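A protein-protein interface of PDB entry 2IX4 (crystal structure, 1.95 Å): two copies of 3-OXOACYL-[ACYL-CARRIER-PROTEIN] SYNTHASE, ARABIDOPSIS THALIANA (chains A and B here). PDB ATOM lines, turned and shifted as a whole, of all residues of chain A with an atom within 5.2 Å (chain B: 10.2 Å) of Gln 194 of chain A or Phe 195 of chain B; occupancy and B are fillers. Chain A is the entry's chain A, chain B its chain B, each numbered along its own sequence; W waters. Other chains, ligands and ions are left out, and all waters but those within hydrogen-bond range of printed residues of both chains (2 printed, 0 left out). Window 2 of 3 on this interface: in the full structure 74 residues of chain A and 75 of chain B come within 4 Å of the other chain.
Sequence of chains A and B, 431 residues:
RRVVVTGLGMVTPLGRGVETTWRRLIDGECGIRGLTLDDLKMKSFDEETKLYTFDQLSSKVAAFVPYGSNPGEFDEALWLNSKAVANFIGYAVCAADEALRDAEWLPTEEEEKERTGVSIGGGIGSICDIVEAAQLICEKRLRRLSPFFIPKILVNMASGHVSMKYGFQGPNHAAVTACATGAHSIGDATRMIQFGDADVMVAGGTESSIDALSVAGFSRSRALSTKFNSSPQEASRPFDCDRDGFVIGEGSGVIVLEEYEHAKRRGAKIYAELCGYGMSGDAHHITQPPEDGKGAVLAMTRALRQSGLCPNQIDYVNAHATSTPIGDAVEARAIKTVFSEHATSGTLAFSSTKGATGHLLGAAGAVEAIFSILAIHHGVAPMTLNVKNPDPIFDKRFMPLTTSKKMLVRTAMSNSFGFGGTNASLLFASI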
ATOM      1  N   ARG A   1     -11.083   9.027  11.902  1.00  0.00           N
ATOM      2  CA  ARG A   1     -11.885   9.564  10.762  1.00  0.00           C
ATOM      3  C   ARG A   1     -11.261   9.140   9.439  1.00  0.00           C
ATOM      4  O   ARG A   1     -10.039   9.218   9.259  1.00  0.00           O
ATOM      5  CB  ARG A   1     -12.000  11.093  10.823  1.00  0.00           C
ATOM      6  CG  ARG A   1     -12.121  11.666  12.234  1.00  0.00           C
ATOM      7  CD  ARG A   1     -12.950  12.937  12.294  1.00  0.00           C
ATOM      8  NE  ARG A   1     -12.488  13.997  11.401  1.00  0.00           N
ATOM      9  CZ  ARG A   1     -13.249  15.007  10.989  1.00  0.00           C
ATOM     10  NH1 ARG A   1     -14.514  15.098  11.387  1.00  0.00           N
ATOM     11  NH2 ARG A   1     -12.755  15.923  10.170  1.00  0.00           N
ATOM     12  N   VAL A   3     -10.969   9.312   5.150  1.00  0.00           N
ATOM     13  CA  VAL A   3     -10.931  10.364   4.134  1.00  0.00           C
ATOM     14  C   VAL A   3     -11.203   9.775   2.753  1.00  0.00           C
ATOM     15  O   VAL A   3     -10.523   8.843   2.319  1.00  0.00           O
ATOM     16  CB  VAL A   3      -9.571  11.118   4.145  1.00  0.00           C
ATOM     17  CG1 VAL A   3      -9.561  12.244   3.116  1.00  0.00           C
ATOM     18  CG2 VAL A   3      -9.274  11.668   5.544  1.00  0.00           C
ATOM     19  N   ALA A 189      -3.350  17.521   3.575  1.00  0.00           N
ATOM     20  CA  ALA A 189      -4.784  17.817   3.638  1.00  0.00           C
ATOM     21  C   ALA A 189      -5.576  16.654   4.238  1.00  0.00           C
ATOM     22  O   ALA A 189      -6.541  16.862   4.982  1.00  0.00           O
ATOM     23  CB  ALA A 189      -5.305  18.157   2.254  1.00  0.00           C
ATOM     24  N   THR A 190      -5.163  15.436   3.902  1.00  0.00           N
ATOM     25  CA  THR A 190      -5.721  14.216   4.485  1.00  0.00           C
ATOM     26  C   THR A 190      -5.512  14.183   6.005  1.00  0.00           C
ATOM     27  O   THR A 190      -6.465  13.959   6.756  1.00  0.00           O
ATOM     28  CB  THR A 190      -5.114  12.967   3.814  1.00  0.00           C
ATOM     29  OG1 THR A 190      -5.429  12.992   2.418  1.00  0.00           O
ATOM     30  CG2 THR A 190      -5.659  11.677   4.424  1.00  0.00           C
ATOM     31  N   ARG A 191      -4.275  14.424   6.446  1.00  0.00           N
ATOM     32  CA  ARG A 191      -3.954  14.502   7.879  1.00  0.00           C
ATOM     33  C   ARG A 191      -4.820  15.519   8.622  1.00  0.00           C
ATOM     34  O   ARG A 191      -5.223  15.283   9.762  1.00  0.00           O
ATOM     35  CB  ARG A 191      -2.475  14.844   8.092  1.00  0.00           C
ATOM     36  CG  ARG A 191      -1.495  13.749   7.710  1.00  0.00           C
ATOM     37  CD  ARG A 191      -1.363  12.682   8.794  1.00  0.00           C
ATOM     38  NE  ARG A 191      -0.431  11.627   8.396  1.00  0.00           N
ATOM     39  CZ  ARG A 191      -0.748  10.599   7.610  1.00  0.00           C
ATOM     40  NH1 ARG A 191      -1.981  10.465   7.133  1.00  0.00           N
ATOM     41  NH2 ARG A 191       0.176   9.697   7.304  1.00  0.00           N
ATOM     42  N   MET A 192      -5.101  16.645   7.968  1.00  0.00           N
ATOM     43  CA  MET A 192      -5.945  17.694   8.537  1.00  0.00           C
ATOM     44  C   MET A 192      -7.396  17.246   8.732  1.00  0.00           C
ATOM     45  O   MET A 192      -7.999  17.537   9.763  1.00  0.00           O
ATOM     46  CB  MET A 192      -5.882  18.969   7.688  1.00  0.00           C
ATOM     47  CG  MET A 192      -4.525  19.661   7.720  1.00  0.00           C
ATOM     48  SD  MET A 192      -4.328  21.002   6.526  1.00  0.00           S
ATOM     49  CE  MET A 192      -2.574  21.323   6.706  1.00  0.00           C
ATOM     50  N   ILE A 193      -7.952  16.550   7.745  1.00  0.00           N
ATOM     51  CA  ILE A 193      -9.307  15.998   7.867  1.00  0.00           C
ATOM     52  C   ILE A 193      -9.343  14.917   8.953  1.00  0.00           C
ATOM     53  O   ILE A 193     -10.272  14.869   9.763  1.00  0.00           O
ATOM     54  CB  ILE A 193      -9.844  15.453   6.514  1.00  0.00           C
ATOM     55  CG1 ILE A 193      -9.913  16.583   5.476  1.00  0.00           C
ATOM     56  CG2 ILE A 193     -11.227  14.816   6.692  1.00  0.00           C
ATOM     57  CD1 ILE A 193     -10.095  16.119   4.039  1.00  0.00           C
ATOM     58  N   GLN A 194      -8.315  14.071   8.969  1.00  0.00           N
ATOM     59  CA  GLN A 194      -8.183  13.010   9.968  1.00  0.00           C
ATOM     60  C   GLN A 194      -8.181  13.571  11.388  1.00  0.00           C
ATOM     61  O   GLN A 194      -8.905  13.075  12.251  1.00  0.00           O
ATOM     62  CB  GLN A 194      -6.913  12.184   9.724  1.00  0.00           C
ATOM     63  CG  GLN A 194      -7.024  11.175   8.588  1.00  0.00           C
ATOM     64  CD  GLN A 194      -5.677  10.593   8.173  1.00  0.00           C
ATOM     65  OE1 GLN A 194      -4.651  11.272   8.203  1.00  0.00           O
ATOM     66  NE2 GLN A 194      -5.682   9.329   7.774  1.00  0.00           N
ATOM     67  N   PHE A 195      -7.375  14.610  11.615  1.00  0.00           N
ATOM     68  CA  PHE A 195      -7.266  15.245  12.933  1.00  0.00           C
ATOM     69  C   PHE A 195      -8.507  16.051  13.314  1.00  0.00           C
ATOM     70  O   PHE A 195      -8.799  16.213  14.497  1.00  0.00           O
ATOM     71  CB  PHE A 195      -6.025  16.138  13.007  1.00  0.00           C
ATOM     72  CG  PHE A 195      -5.650  16.541  14.409  1.00  0.00           C
ATOM     73  CD1 PHE A 195      -4.822  15.731  15.179  1.00  0.00           C
ATOM     74  CD2 PHE A 195      -6.121  17.734  14.958  1.00  0.00           C
ATOM     75  CE1 PHE A 195      -4.469  16.104  16.479  1.00  0.00           C
ATOM     76  CE2 PHE A 195      -5.774  18.114  16.253  1.00  0.00           C
ATOM     77  CZ  PHE A 195      -4.946  17.296  17.014  1.00  0.00           C
ATOM     78  N   GLY A 196      -9.227  16.554  12.315  1.00  0.00           N
ATOM     79  CA  GLY A 196     -10.442  17.338  12.558  1.00  0.00           C
ATOM     80  C   GLY A 196     -10.320  18.827  12.268  1.00  0.00           C
ATOM     81  O   GLY A 196     -11.218  19.600  12.608  1.00  0.00           O
ATOM     82  N   GLN A 306       0.258   1.988   6.990  1.00  0.00           N
ATOM     83  CA  GLN A 306      -0.872   2.830   7.393  1.00  0.00           C
ATOM     84  C   GLN A 306      -2.226   2.266   6.959  1.00  0.00           C
ATOM     85  O   GLN A 306      -3.218   2.394   7.682  1.00  0.00           O
ATOM     86  CB  GLN A 306      -0.716   4.246   6.829  1.00  0.00           C
ATOM     87  CG  GLN A 306       0.371   5.083   7.488  1.00  0.00           C
ATOM     88  CD  GLN A 306       0.683   6.343   6.703  1.00  0.00           C
ATOM     89  OE1 GLN A 306      -0.211   6.967   6.131  1.00  0.00           O
ATOM     90  NE2 GLN A 306       1.957   6.722   6.671  1.00  0.00           N
ATOM     91  N   ARG B   1      -1.033  10.759  20.925  1.00  0.00           N
ATOM     92  CA  ARG B   1       0.377  11.126  20.997  1.00  0.00           C
ATOM     93  C   ARG B   1       0.538  12.621  21.253  1.00  0.00           C
ATOM     94  O   ARG B   1      -0.014  13.447  20.521  1.00  0.00           O
ATOM     95  CB  ARG B   1       1.098  10.747  19.701  1.00  0.00           C
ATOM     96  CG  ARG B   1       1.336   9.257  19.496  1.00  0.00           C
ATOM     97  CD  ARG B   1       2.213   9.037  18.269  1.00  0.00           C
ATOM     98  NE  ARG B   1       3.269   8.068  18.540  1.00  0.00           N
ATOM     99  CZ  ARG B   1       4.492   8.110  18.018  1.00  0.00           C
ATOM    100  NH1 ARG B   1       4.845   9.086  17.185  1.00  0.00           N
ATOM    101  NH2 ARG B   1       5.369   7.172  18.345  1.00  0.00           N
ATOM    102  N   ARG B   2       1.298  12.959  22.291  1.00  0.00           N
ATOM    103  CA  ARG B   2       1.583  14.353  22.622  1.00  0.00           C
ATOM    104  C   ARG B   2       2.953  14.756  22.083  1.00  0.00           C
ATOM    105  O   ARG B   2       3.858  13.922  21.976  1.00  0.00           O
ATOM    106  CB  ARG B   2       1.505  14.580  24.132  1.00  0.00           C
ATOM    107  CG  ARG B   2       0.101  14.434  24.704  1.00  0.00           C
ATOM    108  CD  ARG B   2       0.130  14.306  26.217  1.00  0.00           C
ATOM    109  NE  ARG B   2       0.229  15.598  26.894  1.00  0.00           N
ATOM    110  CZ  ARG B   2       0.338  15.747  28.212  1.00  0.00           C
ATOM    111  NH1 ARG B   2       0.373  14.685  29.009  1.00  0.00           N
ATOM    112  NH2 ARG B   2       0.415  16.962  28.740  1.00  0.00           N
ATOM    113  N   VAL B   3       3.087  16.037  21.746  1.00  0.00           N
ATOM    114  CA  VAL B   3       4.285  16.567  21.091  1.00  0.00           C
ATOM    115  C   VAL B   3       4.913  17.656  21.952  1.00  0.00           C
ATOM    116  O   VAL B   3       4.241  18.608  22.354  1.00  0.00           O
ATOM    117  CB  VAL B   3       3.959  17.128  19.674  1.00  0.00           C
ATOM    118  CG1 VAL B   3       5.211  17.689  18.996  1.00  0.00           C
ATOM    119  CG2 VAL B   3       3.324  16.050  18.804  1.00  0.00           C
ATOM    120  N   ARG B 115      13.191   7.437  12.007  1.00  0.00           N
ATOM    121  CA  ARG B 115      12.054   7.991  12.746  1.00  0.00           C
ATOM    122  C   ARG B 115      12.174   9.504  12.977  1.00  0.00           C
ATOM    123  O   ARG B 115      11.327  10.106  13.642  1.00  0.00           O
ATOM    124  CB  ARG B 115      11.852   7.237  14.070  1.00  0.00           C
ATOM    125  CG  ARG B 115      11.406   5.779  13.907  1.00  0.00           C
ATOM    126  CD  ARG B 115      10.051   5.672  13.205  1.00  0.00           C
ATOM    127  NE  ARG B 115       8.968   6.179  14.041  1.00  0.00           N
ATOM    128  CZ  ARG B 115       7.730   6.410  13.614  1.00  0.00           C
ATOM    129  NH1 ARG B 115       7.400   6.189  12.347  1.00  0.00           N
ATOM    130  NH2 ARG B 115       6.820   6.869  14.459  1.00  0.00           N
ATOM    131  N   PRO B 171       9.815  11.785   7.429  1.00  0.00           N
ATOM    132  CA  PRO B 171       9.198  12.693   6.457  1.00  0.00           C
ATOM    133  C   PRO B 171      10.103  13.885   6.130  1.00  0.00           C
ATOM    134  O   PRO B 171      10.546  14.589   7.041  1.00  0.00           O
ATOM    135  CB  PRO B 171       7.924  13.157   7.172  1.00  0.00           C
ATOM    136  CG  PRO B 171       7.590  12.041   8.106  1.00  0.00           C
ATOM    137  CD  PRO B 171       8.922  11.501   8.569  1.00  0.00           C
ATOM    138  N   GLY B 187       3.713  23.315  12.576  1.00  0.00           N
ATOM    139  CA  GLY B 187       2.405  22.715  12.808  1.00  0.00           C
ATOM    140  C   GLY B 187       2.189  21.409  12.064  1.00  0.00           C
ATOM    141  O   GLY B 187       1.650  20.450  12.626  1.00  0.00           O
ATOM    142  N   ASP B 188       2.601  21.377  10.796  1.00  0.00           N
ATOM    143  CA  ASP B 188       2.520  20.163   9.978  1.00  0.00           C
ATOM    144  C   ASP B 188       3.328  19.037  10.597  1.00  0.00           C
ATOM    145  O   ASP B 188       2.845  17.912  10.703  1.00  0.00           O
ATOM    146  CB  ASP B 188       3.016  20.420   8.554  1.00  0.00           C
ATOM    147  CG  ASP B 188       1.998  21.155   7.696  1.00  0.00           C
ATOM    148  OD1 ASP B 188       0.852  21.376   8.151  1.00  0.00           O
ATOM    149  OD2 ASP B 188       2.352  21.508   6.553  1.00  0.00           O
ATOM    150  N   ALA B 189       4.556  19.355  11.005  1.00  0.00           N
ATOM    151  CA  ALA B 189       5.440  18.397  11.662  1.00  0.00           C
ATOM    152  C   ALA B 189       4.812  17.823  12.928  1.00  0.00           C
ATOM    153  O   ALA B 189       4.971  16.638  13.221  1.00  0.00           O
ATOM    154  CB  ALA B 189       6.774  19.049  11.977  1.00  0.00           C
ATOM    155  N   THR B 190       4.104  18.672  13.672  1.00  0.00           N
ATOM    156  CA  THR B 190       3.369  18.253  14.867  1.00  0.00           C
ATOM    157  C   THR B 190       2.341  17.184  14.517  1.00  0.00           C
ATOM    158  O   THR B 190       2.295  16.133  15.162  1.00  0.00           O
ATOM    159  CB  THR B 190       2.704  19.464  15.583  1.00  0.00           C
ATOM    160  OG1 THR B 190       3.720  20.380  16.003  1.00  0.00           O
ATOM    161  CG2 THR B 190       1.902  19.024  16.809  1.00  0.00           C
ATOM    162  N   ARG B 191       1.539  17.450  13.486  1.00  0.00           N
ATOM    163  CA  ARG B 191       0.523  16.502  13.007  1.00  0.00           C
ATOM    164  C   ARG B 191       1.125  15.150  12.632  1.00  0.00           C
ATOM    165  O   ARG B 191       0.524  14.100  12.877  1.00  0.00           O
ATOM    166  CB  ARG B 191      -0.232  17.081  11.805  1.00  0.00           C
ATOM    167  CG  ARG B 191      -1.139  18.262  12.126  1.00  0.00           C
ATOM    168  CD  ARG B 191      -2.479  17.808  12.697  1.00  0.00           C
ATOM    169  NE  ARG B 191      -3.356  18.942  12.988  1.00  0.00           N
ATOM    170  CZ  ARG B 191      -3.357  19.624  14.132  1.00  0.00           C
ATOM    171  NH1 ARG B 191      -2.532  19.293  15.121  1.00  0.00           N
ATOM    172  NH2 ARG B 191      -4.193  20.641  14.290  1.00  0.00           N
ATOM    173  N   MET B 192       2.314  15.192  12.034  1.00  0.00           N
ATOM    174  CA  MET B 192       3.028  13.990  11.615  1.00  0.00           C
ATOM    175  C   MET B 192       3.453  13.137  12.807  1.00  0.00           C
ATOM    176  O   MET B 192       3.287  11.919  12.786  1.00  0.00           O
ATOM    177  CB  MET B 192       4.235  14.358  10.746  1.00  0.00           C
ATOM    178  CG  MET B 192       3.849  14.965   9.407  1.00  0.00           C
ATOM    179  SD  MET B 192       5.244  15.435   8.374  1.00  0.00           S
ATOM    180  CE  MET B 192       4.352  16.244   7.041  1.00  0.00           C
ATOM    181  N   ILE B 193       3.989  13.778  13.844  1.00  0.00           N
ATOM    182  CA  ILE B 193       4.325  13.073  15.086  1.00  0.00           C
ATOM    183  C   ILE B 193       3.057  12.556  15.769  1.00  0.00           C
ATOM    184  O   ILE B 193       3.015  11.413  16.218  1.00  0.00           O
ATOM    185  CB  ILE B 193       5.158  13.946  16.051  1.00  0.00           C
ATOM    186  CG1 ILE B 193       6.465  14.382  15.378  1.00  0.00           C
ATOM    187  CG2 ILE B 193       5.466  13.187  17.340  1.00  0.00           C
ATOM    188  CD1 ILE B 193       7.199  15.486  16.110  1.00  0.00           C
ATOM    189  N   GLN B 194       2.020  13.393  15.815  1.00  0.00           N
ATOM    190  CA  GLN B 194       0.730  13.009  16.394  1.00  0.00           C
ATOM    191  C   GLN B 194       0.163  11.748  15.744  1.00  0.00           C
ATOM    192  O   GLN B 194      -0.321  10.849  16.440  1.00  0.00           O
ATOM    193  CB  GLN B 194      -0.283  14.155  16.279  1.00  0.00           C
ATOM    194  CG  GLN B 194      -0.067  15.295  17.268  1.00  0.00           C
ATOM    195  CD  GLN B 194      -0.952  16.498  16.986  1.00  0.00           C
ATOM    196  OE1 GLN B 194      -1.212  16.842  15.831  1.00  0.00           O
ATOM    197  NE2 GLN B 194      -1.420  17.145  18.045  1.00  0.00           N
ATOM    198  N   PHE B 195       0.234  11.686  14.415  1.00  0.00           N
ATOM    199  CA  PHE B 195      -0.298  10.553  13.658  1.00  0.00           C
ATOM    200  C   PHE B 195       0.584   9.305  13.745  1.00  0.00           C
ATOM    201  O   PHE B 195       0.081   8.181  13.689  1.00  0.00           O
ATOM    202  CB  PHE B 195      -0.523  10.938  12.193  1.00  0.00           C
ATOM    203  CG  PHE B 195      -1.329   9.930  11.422  1.00  0.00           C
ATOM    204  CD1 PHE B 195      -2.722   9.935  11.491  1.00  0.00           C
ATOM    205  CD2 PHE B 195      -0.700   8.973  10.630  1.00  0.00           C
ATOM    206  CE1 PHE B 195      -3.474   8.997  10.783  1.00  0.00           C
ATOM    207  CE2 PHE B 195      -1.445   8.033   9.919  1.00  0.00           C
ATOM    208  CZ  PHE B 195      -2.832   8.045   9.995  1.00  0.00           C
ATOM    209  N   GLY B 196       1.893   9.504  13.873  1.00  0.00           N
ATOM    210  CA  GLY B 196       2.836   8.392  13.967  1.00  0.00           C
ATOM    211  C   GLY B 196       3.758   8.282  12.768  1.00  0.00           C
ATOM    212  O   GLY B 196       4.442   7.269  12.601  1.00  0.00           O
ATOM    213  N   ASP B 197       3.781   9.321  11.934  1.00  0.00           N
ATOM    214  CA  ASP B 197       4.670   9.378  10.768  1.00  0.00           C
ATOM    215  C   ASP B 197       6.132   9.477  11.189  1.00  0.00           C
ATOM    216  O   ASP B 197       7.025   9.042  10.460  1.00  0.00           O
ATOM    217  CB  ASP B 197       4.326  10.575   9.883  1.00  0.00           C
ATOM    218  CG  ASP B 197       2.945  10.470   9.262  1.00  0.00           C
ATOM    219  OD1 ASP B 197       2.658   9.450   8.595  1.00  0.00           O
ATOM    220  OD2 ASP B 197       2.151  11.420   9.422  1.00  0.00           O
ATOM    221  N   ALA B 198       6.360  10.067  12.360  1.00  0.00           N
ATOM    222  CA  ALA B 198       7.701  10.262  12.907  1.00  0.00           C
ATOM    223  C   ALA B 198       7.647  10.357  14.424  1.00  0.00           C
ATOM    224  O   ALA B 198       6.587  10.603  14.998  1.00  0.00           O
ATOM    225  CB  ALA B 198       8.326  11.524  12.330  1.00  0.00           C
ATOM    226  N   ASP B 199       8.794  10.161  15.067  1.00  0.00           N
ATOM    227  CA  ASP B 199       8.918  10.349  16.508  1.00  0.00           C
ATOM    228  C   ASP B 199       9.611  11.668  16.823  1.00  0.00           C
ATOM    229  O   ASP B 199       9.417  12.239  17.892  1.00  0.00           O
ATOM    230  CB  ASP B 199       9.693   9.189  17.142  1.00  0.00           C
ATOM    231  CG  ASP B 199       8.933   7.880  17.080  1.00  0.00           C
ATOM    232  OD1 ASP B 199       7.681   7.906  17.135  1.00  0.00           O
ATOM    233  OD2 ASP B 199       9.594   6.823  16.978  1.00  0.00           O
ATOM    234  N   MET B 201      10.830  15.477  14.803  1.00  0.00           N
ATOM    235  CA  MET B 201      10.812  16.359  13.639  1.00  0.00           C
ATOM    236  C   MET B 201      11.651  17.608  13.890  1.00  0.00           C
ATOM    237  O   MET B 201      11.500  18.275  14.916  1.00  0.00           O
ATOM    238  CB  MET B 201       9.377  16.748  13.256  1.00  0.00           C
ATOM    239  CG  MET B 201       8.532  15.619  12.637  1.00  0.00           C
ATOM    240  SD  MET B 201       9.085  14.996  11.027  1.00  0.00           S
ATOM    241  CE  MET B 201       8.678  16.374   9.952  1.00  0.00           C
ATOM    242  N   GLU B 259       7.864  13.288  20.200  1.00  0.00           N
ATOM    243  CA  GLU B 259       6.767  12.592  20.864  1.00  0.00           C
ATOM    244  C   GLU B 259       7.076  12.513  22.361  1.00  0.00           C
ATOM    245  O   GLU B 259       8.214  12.235  22.752  1.00  0.00           O
ATOM    246  CB  GLU B 259       6.553  11.204  20.253  1.00  0.00           C
ATOM    247  CG  GLU B 259       5.270  10.501  20.688  1.00  0.00           C
ATOM    248  CD  GLU B 259       5.449   9.695  21.962  1.00  0.00           C
ATOM    249  OE1 GLU B 259       6.539   9.107  22.150  1.00  0.00           O
ATOM    250  OE2 GLU B 259       4.503   9.648  22.776  1.00  0.00           O
ATOM    251  N   MET B 279      -5.634  26.766  12.144  1.00  0.00           N
ATOM    252  CA  MET B 279      -5.454  27.166  10.754  1.00  0.00           C
ATOM    253  C   MET B 279      -6.747  27.721  10.193  1.00  0.00           C
ATOM    254  O   MET B 279      -7.823  27.190  10.457  1.00  0.00           O
ATOM    255  CB  MET B 279      -5.019  25.976   9.899  1.00  0.00           C
ATOM    256  CG  MET B 279      -3.625  25.449  10.178  1.00  0.00           C
ATOM    257  SD  MET B 279      -3.299  24.000   9.166  1.00  0.00           S
ATOM    258  CE  MET B 279      -4.269  22.762  10.018  1.00  0.00           C
HETATM  259  O   HOH W   1       4.763   8.380   6.684  1.00  0.00           O
HETATM  260  O   HOH W   2       2.175   6.902   9.829  1.00  0.00           O
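The guanidinium group (NE) of Arg 191 of chain A lies within salt-bridge range of the side-chain carboxylate (OD2) of Asp 197 of chain B.
NE2 of Gln 306 of chain A sits at hydrogen-bond distance from OD1 of Asp 197 of chain B.
O of Met 192 of chain B is in hydrogen-bond range of N of Asp 197 of chain B, at 2.8 Å.
The guanidinium group (NH1) of Arg 191 of chain A sits at hydrogen-bond distance from the side-chain amide oxygen (OE1) of Gln 194 of chain A (3.0 Å).
OE1 of Gln 194 of chain B is in hydrogen-bond range of NH1 of Arg 191 of chain B, 2.9 Å away.
The guanidinium group (NH1) of Arg 115 of chain B sits at hydrogen-bond distance from the backbone carbonyl oxygen (O) of Asp 197 of chain B, 3.4 Å away.
NH2 of Arg 191 of chain A sits at hydrogen-bond distance from OE1 of Gln 306 of chain A (3.0 Å).
Among the printed residues, pairs that only touch across the chains: Arg 191 of chain A with Phe 195 of chain B (3.4 Å), Met 192 of chain A with Asp 188 of chain B (3.7 Å), Met 192 of chain A with Met 279 of chain B (3.7 Å), Gln 194 of chain A with Phe 195 of chain B (3.6 Å), Phe 195 of chain A with Arg 191 of chain B (3.4 Å) and Phe 195 of chain A with Gln 194 of chain B (3.4 Å).
Gln 194 of chain A touches one residue of chain B.
Phe 195 of chain B touches two residues of chain A.
Of the printed residues of chain A, Gln 194 of chain B touches Phe 195 (3.4 Å).
Of the printed residues of chain B, Phe 195 of chain A touches Arg 191 and Gln 194.
Printed residues of chain A within 4 Å of Asp 197 of chain B: Arg 191 and Gln 306.
Printed residues of chain B within 4 Å of Gln 306 of chain A: Asp 197.
Of the printed residues of chain A, Arg 191 of chain B touches Phe 195.
Met 201 of chain B touches none of the printed residues of chain A.
Gly 187 of chain B touches none of the printed residues of chain A.
The nearest residue of chain A that does not touch Phe 195 of chain B is Gln 306 of chain A (4.1 Å).
Of the 11 printed residues of chain A, 5 touch a printed residue of chain B.
Hydrophobic or aromatic side chains of chain A that line the printed part of chain B: Met 192 and Phe 195.
Hydrophobic or aromatic side chains of chain B that line the printed part of chain A: Phe 195 and Met 279.
Among the printed residues, Asp or Glu carboxylates within 4 Å of a Lys or Arg side-chain nitrogen of the other chain: Arg 191 of chain A with Asp 197 of chain B (2.8 Å).
Arg 191 of chain A touches Phe 195 of chain B, and with the chains exchanged Phe 195 of chain A touches Arg 191 of chain B.
Gln 194 of chain A touches Phe 195 of chain B, and with the chains exchanged Phe 195 of chain A touches Gln 194 of chain B.
Positions printed for both chains: 1, 3, 189, 190, 191, 192, 193, 194, 195 and 196.
Of the 8 pairs that touch across the chains among the printed residues, 4 have their exchanged pair printed and touching as well.
Water W2 lies within hydrogen-bond range of OD1 of Asp 197 of chain B and NE2 of Gln 306 of chain A.
Water W1 bridges OD1 of Asp 197 of chain B (3.0 Å) and NE2 of Gln 306 of chain A (3.3 Å).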
